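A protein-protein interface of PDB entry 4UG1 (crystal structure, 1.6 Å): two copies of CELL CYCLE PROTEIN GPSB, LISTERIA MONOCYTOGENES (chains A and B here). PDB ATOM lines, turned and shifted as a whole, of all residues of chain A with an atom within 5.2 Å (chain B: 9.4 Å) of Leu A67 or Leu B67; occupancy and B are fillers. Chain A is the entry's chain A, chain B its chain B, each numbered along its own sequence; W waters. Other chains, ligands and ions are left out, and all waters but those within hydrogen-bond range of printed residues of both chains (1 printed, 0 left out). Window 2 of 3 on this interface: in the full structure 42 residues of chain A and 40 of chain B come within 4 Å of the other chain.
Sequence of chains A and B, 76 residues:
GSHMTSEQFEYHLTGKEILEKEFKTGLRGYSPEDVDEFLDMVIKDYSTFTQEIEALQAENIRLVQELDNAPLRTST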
ATOM      1  N   LEU A  63     -16.055 -24.115 -10.363  1.00  0.00           N
ATOM      2  CA  LEU A  63     -16.636 -22.812 -10.666  1.00  0.00           C
ATOM      3  C   LEU A  63     -17.722 -22.446  -9.661  1.00  0.00           C
ATOM      4  O   LEU A  63     -17.782 -21.308  -9.188  1.00  0.00           O
ATOM      5  CB  LEU A  63     -17.202 -22.799 -12.088  1.00  0.00           C
ATOM      6  CG  LEU A  63     -16.102 -22.922 -13.142  1.00  0.00           C
ATOM      7  CD1 LEU A  63     -16.727 -23.226 -14.490  1.00  0.00           C
ATOM      8  CD2 LEU A  63     -15.273 -21.664 -13.198  1.00  0.00           C
ATOM      9  N   VAL A  64     -18.578 -23.413  -9.346  1.00  0.00           N
ATOM     10  CA  VAL A  64     -19.625 -23.196  -8.351  1.00  0.00           C
ATOM     11  C   VAL A  64     -19.019 -22.794  -7.006  1.00  0.00           C
ATOM     12  O   VAL A  64     -19.514 -21.882  -6.329  1.00  0.00           O
ATOM     13  CB  VAL A  64     -20.507 -24.458  -8.180  1.00  0.00           C
ATOM     14  CG1 VAL A  64     -21.468 -24.283  -7.009  1.00  0.00           C
ATOM     15  CG2 VAL A  64     -21.278 -24.736  -9.456  1.00  0.00           C
ATOM     16  N   GLN A  65     -17.923 -23.448  -6.631  1.00  0.00           N
ATOM     17  CA  GLN A  65     -17.294 -23.189  -5.337  1.00  0.00           C
ATOM     18  C   GLN A  65     -16.608 -21.824  -5.301  1.00  0.00           C
ATOM     19  O   GLN A  65     -16.541 -21.186  -4.257  1.00  0.00           O
ATOM     20  CB  GLN A  65     -16.311 -24.314  -5.000  1.00  0.00           C
ATOM     21  CG  GLN A  65     -17.020 -25.616  -4.644  1.00  0.00           C
ATOM     22  CD  GLN A  65     -16.085 -26.706  -4.157  1.00  0.00           C
ATOM     23  OE1 GLN A  65     -14.866 -26.576  -4.231  1.00  0.00           O
ATOM     24  NE2 GLN A  65     -16.659 -27.795  -3.657  1.00  0.00           N
ATOM     25  N   GLU A  66     -16.112 -21.366  -6.447  1.00  0.00           N
ATOM     26  CA  GLU A  66     -15.611 -19.999  -6.556  1.00  0.00           C
ATOM     27  C   GLU A  66     -16.740 -18.999  -6.338  1.00  0.00           C
ATOM     28  O   GLU A  66     -16.568 -18.006  -5.643  1.00  0.00           O
ATOM     29  CB  GLU A  66     -14.963 -19.751  -7.917  1.00  0.00           C
ATOM     30  CG  GLU A  66     -13.630 -20.446  -8.118  1.00  0.00           C
ATOM     31  CD  GLU A  66     -12.793 -19.776  -9.194  1.00  0.00           C
ATOM     32  OE1 GLU A  66     -12.165 -18.734  -8.905  1.00  0.00           O
ATOM     33  OE2 GLU A  66     -12.783 -20.280 -10.334  1.00  0.00           O
ATOM     34  N   LEU A  67     -17.894 -19.274  -6.938  1.00  0.00           N
ATOM     35  CA  LEU A  67     -19.035 -18.371  -6.830  1.00  0.00           C
ATOM     36  C   LEU A  67     -19.632 -18.387  -5.431  1.00  0.00           C
ATOM     37  O   LEU A  67     -20.367 -17.475  -5.059  1.00  0.00           O
ATOM     38  CB  LEU A  67     -20.103 -18.728  -7.869  1.00  0.00           C
ATOM     39  CG  LEU A  67     -19.702 -18.376  -9.305  1.00  0.00           C
ATOM     40  CD1 LEU A  67     -20.544 -19.143 -10.330  1.00  0.00           C
ATOM     41  CD2 LEU A  67     -19.789 -16.869  -9.527  1.00  0.00           C
ATOM     42  N   ASP A  68     -19.308 -19.411  -4.647  1.00  0.00           N
ATOM     43  CA  ASP A  68     -19.705 -19.432  -3.235  1.00  0.00           C
ATOM     44  C   ASP A  68     -19.168 -18.231  -2.470  1.00  0.00           C
ATOM     45  O   ASP A  68     -19.724 -17.848  -1.440  1.00  0.00           O
ATOM     46  CB  ASP A  68     -19.223 -20.708  -2.543  1.00  0.00           C
ATOM     47  CG  ASP A  68     -20.149 -21.878  -2.767  1.00  0.00           C
ATOM     48  OD1 ASP A  68     -21.345 -21.650  -3.047  1.00  0.00           O
ATOM     49  OD2 ASP A  68     -19.675 -23.029  -2.658  1.00  0.00           O
ATOM     50  N   ASN A  69     -18.078 -17.649  -2.965  1.00  0.00           N
ATOM     51  CA  ASN A  69     -17.453 -16.519  -2.290  1.00  0.00           C
ATOM     52  C   ASN A  69     -17.879 -15.175  -2.864  1.00  0.00           C
ATOM     53  O   ASN A  69     -17.306 -14.145  -2.525  1.00  0.00           O
ATOM     54  CB  ASN A  69     -15.927 -16.635  -2.353  1.00  0.00           C
ATOM     55  CG  ASN A  69     -15.400 -17.856  -1.620  1.00  0.00           C
ATOM     56  OD1 ASN A  69     -15.798 -18.138  -0.490  1.00  0.00           O
ATOM     57  ND2 ASN A  69     -14.496 -18.587  -2.263  1.00  0.00           N
ATOM     58  N   ALA A  70     -18.881 -15.182  -3.737  1.00  0.00           N
ATOM     59  CA  ALA A  70     -19.344 -13.941  -4.352  1.00  0.00           C
ATOM     60  C   ALA A  70     -20.344 -13.220  -3.454  1.00  0.00           C
ATOM     61  O   ALA A  70     -21.170 -13.854  -2.801  1.00  0.00           O
ATOM     62  CB  ALA A  70     -19.955 -14.218  -5.712  1.00  0.00           C
ATOM     63  N   GLU B  59     -23.061 -25.414 -19.503  1.00  0.00           N
ATOM     64  CA  GLU B  59     -23.238 -24.957 -18.138  1.00  0.00           C
ATOM     65  C   GLU B  59     -21.978 -24.297 -17.610  1.00  0.00           C
ATOM     66  O   GLU B  59     -22.044 -23.209 -17.024  1.00  0.00           O
ATOM     67  CB  GLU B  59     -23.633 -26.105 -17.223  1.00  0.00           C
ATOM     68  CG  GLU B  59     -23.895 -25.615 -15.817  1.00  0.00           C
ATOM     69  CD  GLU B  59     -24.186 -26.739 -14.858  1.00  0.00           C
ATOM     70  OE1 GLU B  59     -24.348 -27.886 -15.321  1.00  0.00           O
ATOM     71  OE2 GLU B  59     -24.235 -26.467 -13.637  1.00  0.00           O
ATOM     72  N   ASN B  60     -20.832 -24.927 -17.842  1.00  0.00           N
ATOM     73  CA  ASN B  60     -19.584 -24.363 -17.341  1.00  0.00           C
ATOM     74  C   ASN B  60     -19.280 -22.997 -17.971  1.00  0.00           C
ATOM     75  O   ASN B  60     -18.786 -22.097 -17.298  1.00  0.00           O
ATOM     76  CB  ASN B  60     -18.439 -25.343 -17.573  1.00  0.00           C
ATOM     77  CG  ASN B  60     -18.504 -26.551 -16.631  1.00  0.00           C
ATOM     78  OD1 ASN B  60     -19.240 -26.556 -15.640  1.00  0.00           O
ATOM     79  ND2 ASN B  60     -17.705 -27.567 -16.930  1.00  0.00           N
ATOM     80  N   ILE B  61     -19.610 -22.829 -19.250  1.00  0.00           N
ATOM     81  CA  ILE B  61     -19.389 -21.547 -19.905  1.00  0.00           C
ATOM     82  C   ILE B  61     -20.268 -20.458 -19.287  1.00  0.00           C
ATOM     83  O   ILE B  61     -19.814 -19.323 -19.082  1.00  0.00           O
ATOM     84  CB  ILE B  61     -19.637 -21.659 -21.416  1.00  0.00           C
ATOM     85  CG1 ILE B  61     -18.450 -22.364 -22.068  1.00  0.00           C
ATOM     86  CG2 ILE B  61     -19.838 -20.278 -22.036  1.00  0.00           C
ATOM     87  CD1 ILE B  61     -18.746 -22.949 -23.432  1.00  0.00           C
ATOM     88  N   ARG B  62     -21.514 -20.810 -18.973  1.00  0.00           N
ATOM     89  CA  ARG B  62     -22.388 -19.899 -18.233  1.00  0.00           C
ATOM     90  C   ARG B  62     -21.783 -19.496 -16.888  1.00  0.00           C
ATOM     91  O   ARG B  62     -21.864 -18.326 -16.476  1.00  0.00           O
ATOM     92  CB  ARG B  62     -23.764 -20.538 -18.005  1.00  0.00           C
ATOM     93  CG  ARG B  62     -24.630 -20.638 -19.251  1.00  0.00           C
ATOM     94  CD  ARG B  62     -26.075 -20.993 -18.903  1.00  0.00           C
ATOM     95  NE  ARG B  62     -26.227 -22.344 -18.354  1.00  0.00           N
ATOM     96  CZ  ARG B  62     -26.414 -23.436 -19.094  1.00  0.00           C
ATOM     97  NH1 ARG B  62     -26.463 -23.349 -20.415  1.00  0.00           N
ATOM     98  NH2 ARG B  62     -26.547 -24.619 -18.514  1.00  0.00           N
ATOM     99  N   LEU B  63     -21.173 -20.462 -16.206  1.00  0.00           N
ATOM    100  CA  LEU B  63     -20.637 -20.190 -14.888  1.00  0.00           C
ATOM    101  C   LEU B  63     -19.401 -19.302 -14.982  1.00  0.00           C
ATOM    102  O   LEU B  63     -19.214 -18.426 -14.149  1.00  0.00           O
ATOM    103  CB  LEU B  63     -20.313 -21.492 -14.154  1.00  0.00           C
ATOM    104  CG  LEU B  63     -21.525 -22.326 -13.750  1.00  0.00           C
ATOM    105  CD1 LEU B  63     -21.093 -23.694 -13.257  1.00  0.00           C
ATOM    106  CD2 LEU B  63     -22.311 -21.583 -12.684  1.00  0.00           C
ATOM    107  N   VAL B  64     -18.562 -19.521 -15.994  1.00  0.00           N
ATOM    108  CA  VAL B  64     -17.373 -18.682 -16.168  1.00  0.00           C
ATOM    109  C   VAL B  64     -17.767 -17.234 -16.463  1.00  0.00           C
ATOM    110  O   VAL B  64     -17.130 -16.288 -15.988  1.00  0.00           O
ATOM    111  CB  VAL B  64     -16.461 -19.213 -17.298  1.00  0.00           C
ATOM    112  CG1 VAL B  64     -15.320 -18.236 -17.569  1.00  0.00           C
ATOM    113  CG2 VAL B  64     -15.901 -20.575 -16.925  1.00  0.00           C
ATOM    114  N   GLN B  65     -18.828 -17.063 -17.247  1.00  0.00           N
ATOM    115  CA  GLN B  65     -19.352 -15.734 -17.548  1.00  0.00           C
ATOM    116  C   GLN B  65     -19.820 -15.037 -16.275  1.00  0.00           C
ATOM    117  O   GLN B  65     -19.546 -13.850 -16.062  1.00  0.00           O
ATOM    118  CB  GLN B  65     -20.494 -15.837 -18.565  1.00  0.00           C
ATOM    119  CG  GLN B  65     -20.022 -16.181 -19.970  1.00  0.00           C
ATOM    120  CD  GLN B  65     -21.162 -16.476 -20.927  1.00  0.00           C
ATOM    121  OE1 GLN B  65     -22.328 -16.522 -20.532  1.00  0.00           O
ATOM    122  NE2 GLN B  65     -20.829 -16.677 -22.196  1.00  0.00           N
ATOM    123  N   GLU B  66     -20.507 -15.790 -15.424  1.00  0.00           N
ATOM    124  CA  GLU B  66     -20.954 -15.283 -14.133  1.00  0.00           C
ATOM    125  C   GLU B  66     -19.758 -14.892 -13.264  1.00  0.00           C
ATOM    126  O   GLU B  66     -19.759 -13.825 -12.628  1.00  0.00           O
ATOM    127  CB  GLU B  66     -21.817 -16.335 -13.434  1.00  0.00           C
ATOM    128  CG  GLU B  66     -22.794 -15.800 -12.404  1.00  0.00           C
ATOM    129  CD  GLU B  66     -23.817 -16.846 -11.981  1.00  0.00           C
ATOM    130  OE1 GLU B  66     -23.989 -17.846 -12.710  1.00  0.00           O
ATOM    131  OE2 GLU B  66     -24.448 -16.675 -10.917  1.00  0.00           O
ATOM    132  N   LEU B  67     -18.725 -15.735 -13.261  1.00  0.00           N
ATOM    133  CA  LEU B  67     -17.543 -15.484 -12.439  1.00  0.00           C
ATOM    134  C   LEU B  67     -16.732 -14.275 -12.912  1.00  0.00           C
ATOM    135  O   LEU B  67     -16.179 -13.547 -12.089  1.00  0.00           O
ATOM    136  CB  LEU B  67     -16.655 -16.733 -12.412  1.00  0.00           C
ATOM    137  CG  LEU B  67     -15.498 -16.728 -11.403  1.00  0.00           C
ATOM    138  CD1 LEU B  67     -16.006 -16.526  -9.981  1.00  0.00           C
ATOM    139  CD2 LEU B  67     -14.744 -18.038 -11.522  1.00  0.00           C
ATOM    140  N   ASP B  68     -16.650 -14.072 -14.227  1.00  0.00           N
ATOM    141  CA  ASP B  68     -15.942 -12.916 -14.789  1.00  0.00           C
ATOM    142  C   ASP B  68     -16.447 -11.618 -14.193  1.00  0.00           C
ATOM    143  O   ASP B  68     -15.675 -10.690 -13.941  1.00  0.00           O
ATOM    144  CB  ASP B  68     -16.112 -12.833 -16.311  1.00  0.00           C
ATOM    145  CG  ASP B  68     -15.292 -13.855 -17.060  1.00  0.00           C
ATOM    146  OD1 ASP B  68     -14.445 -14.524 -16.434  1.00  0.00           O
ATOM    147  OD2 ASP B  68     -15.497 -13.975 -18.289  1.00  0.00           O
ATOM    148  N   ASN B  69     -17.754 -11.553 -13.972  1.00  0.00           N
ATOM    149  CA  ASN B  69     -18.374 -10.317 -13.519  1.00  0.00           C
ATOM    150  C   ASN B  69     -18.473 -10.189 -11.998  1.00  0.00           C
ATOM    151  O   ASN B  69     -18.838  -9.133 -11.488  1.00  0.00           O
ATOM    152  CB  ASN B  69     -19.770 -10.191 -14.139  1.00  0.00           C
ATOM    153  CG  ASN B  69     -20.352  -8.798 -13.998  1.00  0.00           C
ATOM    154  OD1 ASN B  69     -19.710  -7.798 -14.334  1.00  0.00           O
ATOM    155  ND2 ASN B  69     -21.573  -8.722 -13.485  1.00  0.00           N
ATOM    156  N   ALA B  70     -18.133 -11.255 -11.281  1.00  0.00           N
ATOM    157  CA  ALA B  70     -18.361 -11.329  -9.840  1.00  0.00           C
ATOM    158  C   ALA B  70     -17.222 -10.771  -8.979  1.00  0.00           C
ATOM    159  O   ALA B  70     -16.068 -11.182  -9.117  1.00  0.00           O
ATOM    160  CB  ALA B  70     -18.624 -12.775  -9.448  1.00  0.00           C
ATOM    161  N   PRO B  71     -17.547  -9.852  -8.061  1.00  0.00           N
ATOM    162  CA  PRO B  71     -16.532  -9.464  -7.078  1.00  0.00           C
ATOM    163  C   PRO B  71     -16.347 -10.569  -6.040  1.00  0.00           C
ATOM    164  O   PRO B  71     -17.324 -11.227  -5.698  1.00  0.00           O
ATOM    165  CB  PRO B  71     -17.111  -8.193  -6.440  1.00  0.00           C
ATOM    166  CG  PRO B  71     -18.491  -8.018  -7.021  1.00  0.00           C
ATOM    167  CD  PRO B  71     -18.855  -9.230  -7.797  1.00  0.00           C
ATOM    168  N   LEU B  72     -15.122 -10.773  -5.558  1.00  0.00           N
ATOM    169  CA  LEU B  72     -14.858 -11.816  -4.573  1.00  0.00           C
ATOM    170  C   LEU B  72     -14.416 -11.241  -3.230  1.00  0.00           C
ATOM    171  O   LEU B  72     -14.984 -11.574  -2.188  1.00  0.00           O
ATOM    172  CB  LEU B  72     -13.798 -12.785  -5.098  1.00  0.00           C
ATOM    173  CG  LEU B  72     -14.138 -13.463  -6.434  1.00  0.00           C
ATOM    174  CD1 LEU B  72     -13.060 -14.453  -6.875  1.00  0.00           C
ATOM    175  CD2 LEU B  72     -15.517 -14.142  -6.380  1.00  0.00           C
HETATM  176  O   HOH W   1     -18.313 -11.039  -2.093  1.00  0.00           O
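O of Leu B72 lies close to O of Asn A69, 3.5 Å away.
Hydrophobic or aromatic side chains of chain B within 4 Å of the printed part of chain A: Leu B63, Val B64 and Leu B67. Printed residues of chain A that touch a printed residue of chain B: Leu A63, Val A64, Glu A66, Leu A67, Asn A69 and Ala A70. Hydrophobic or aromatic side chains of chain A within 4 Å of the printed part of chain B: Leu A63, Val A64, Leu A67 and Ala A70. Among the printed residues, no Asp or Glu carboxylate lies within 4 Å of a Lys or Arg side-chain nitrogen of the other chain.
Leu A63 touches its own counterpart, Leu B63. Leu A63 touches Val B64, and with the chains exchanged Val A64 touches Leu B63. Leu A67 touches Leu B63, but with the chains exchanged Leu A63 does not touch Leu B67 (4.03 Å). Leu A67 touches its own counterpart, Leu B67. Of the 9 pairs that touch across the chains among the printed residues, 4 have their exchanged pair printed and touching as well.
Of chain B, only Leu B63 (3.8 Å) and Leu B67 (3.8 Å) come within 4 Å of Leu A67. Of chain A, only Glu A66 and Leu A67 come within 4 Å of Leu B67. Glu A66 touches just one residue of chain B: Leu B67. Printed residues of chain B within 4 Å of Asn A69: Leu B72 (3.5 Å). Printed residues of chain A within 4 Å of Leu B63: Leu A63, Val A64 and Leu A67. Printed residues of chain A within 4 Å of Pro B71: Ala A70 (3.6 Å). Printed residues of chain A within 4 Å of Leu B72: Asn A69 (3.5 Å). Asn B69 touches none of the printed residues of chain A. The nearest residue of chain A that does not touch Leu B67 is Leu A63 (4.03 Å). The nearest printed residue of chain A that does not touch Leu B63 is Gln A65 (7.3 Å).
Water W1 bridges the backbone carbonyl oxygen (O) of Asn A69 (3.3 Å) and the backbone carbonyl oxygen (O) of Leu B72 (3.4 Å).
Leu A63 touches Asn B60 (CD1 to O, 3.7 Å). CB of Leu B63 touches CB of Leu A63, 3.96 Å away. Val B64 touches Leu A63 (CG2 to CD1, 3.7 Å). Leu B63 touches Val A64 (CD1 to CG2, 3.9 Å). Glu A66 touches Leu B67. Leu B63 touches Leu A67. Leu A67 touches Leu B67. Pro B71 touches Ala A70.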
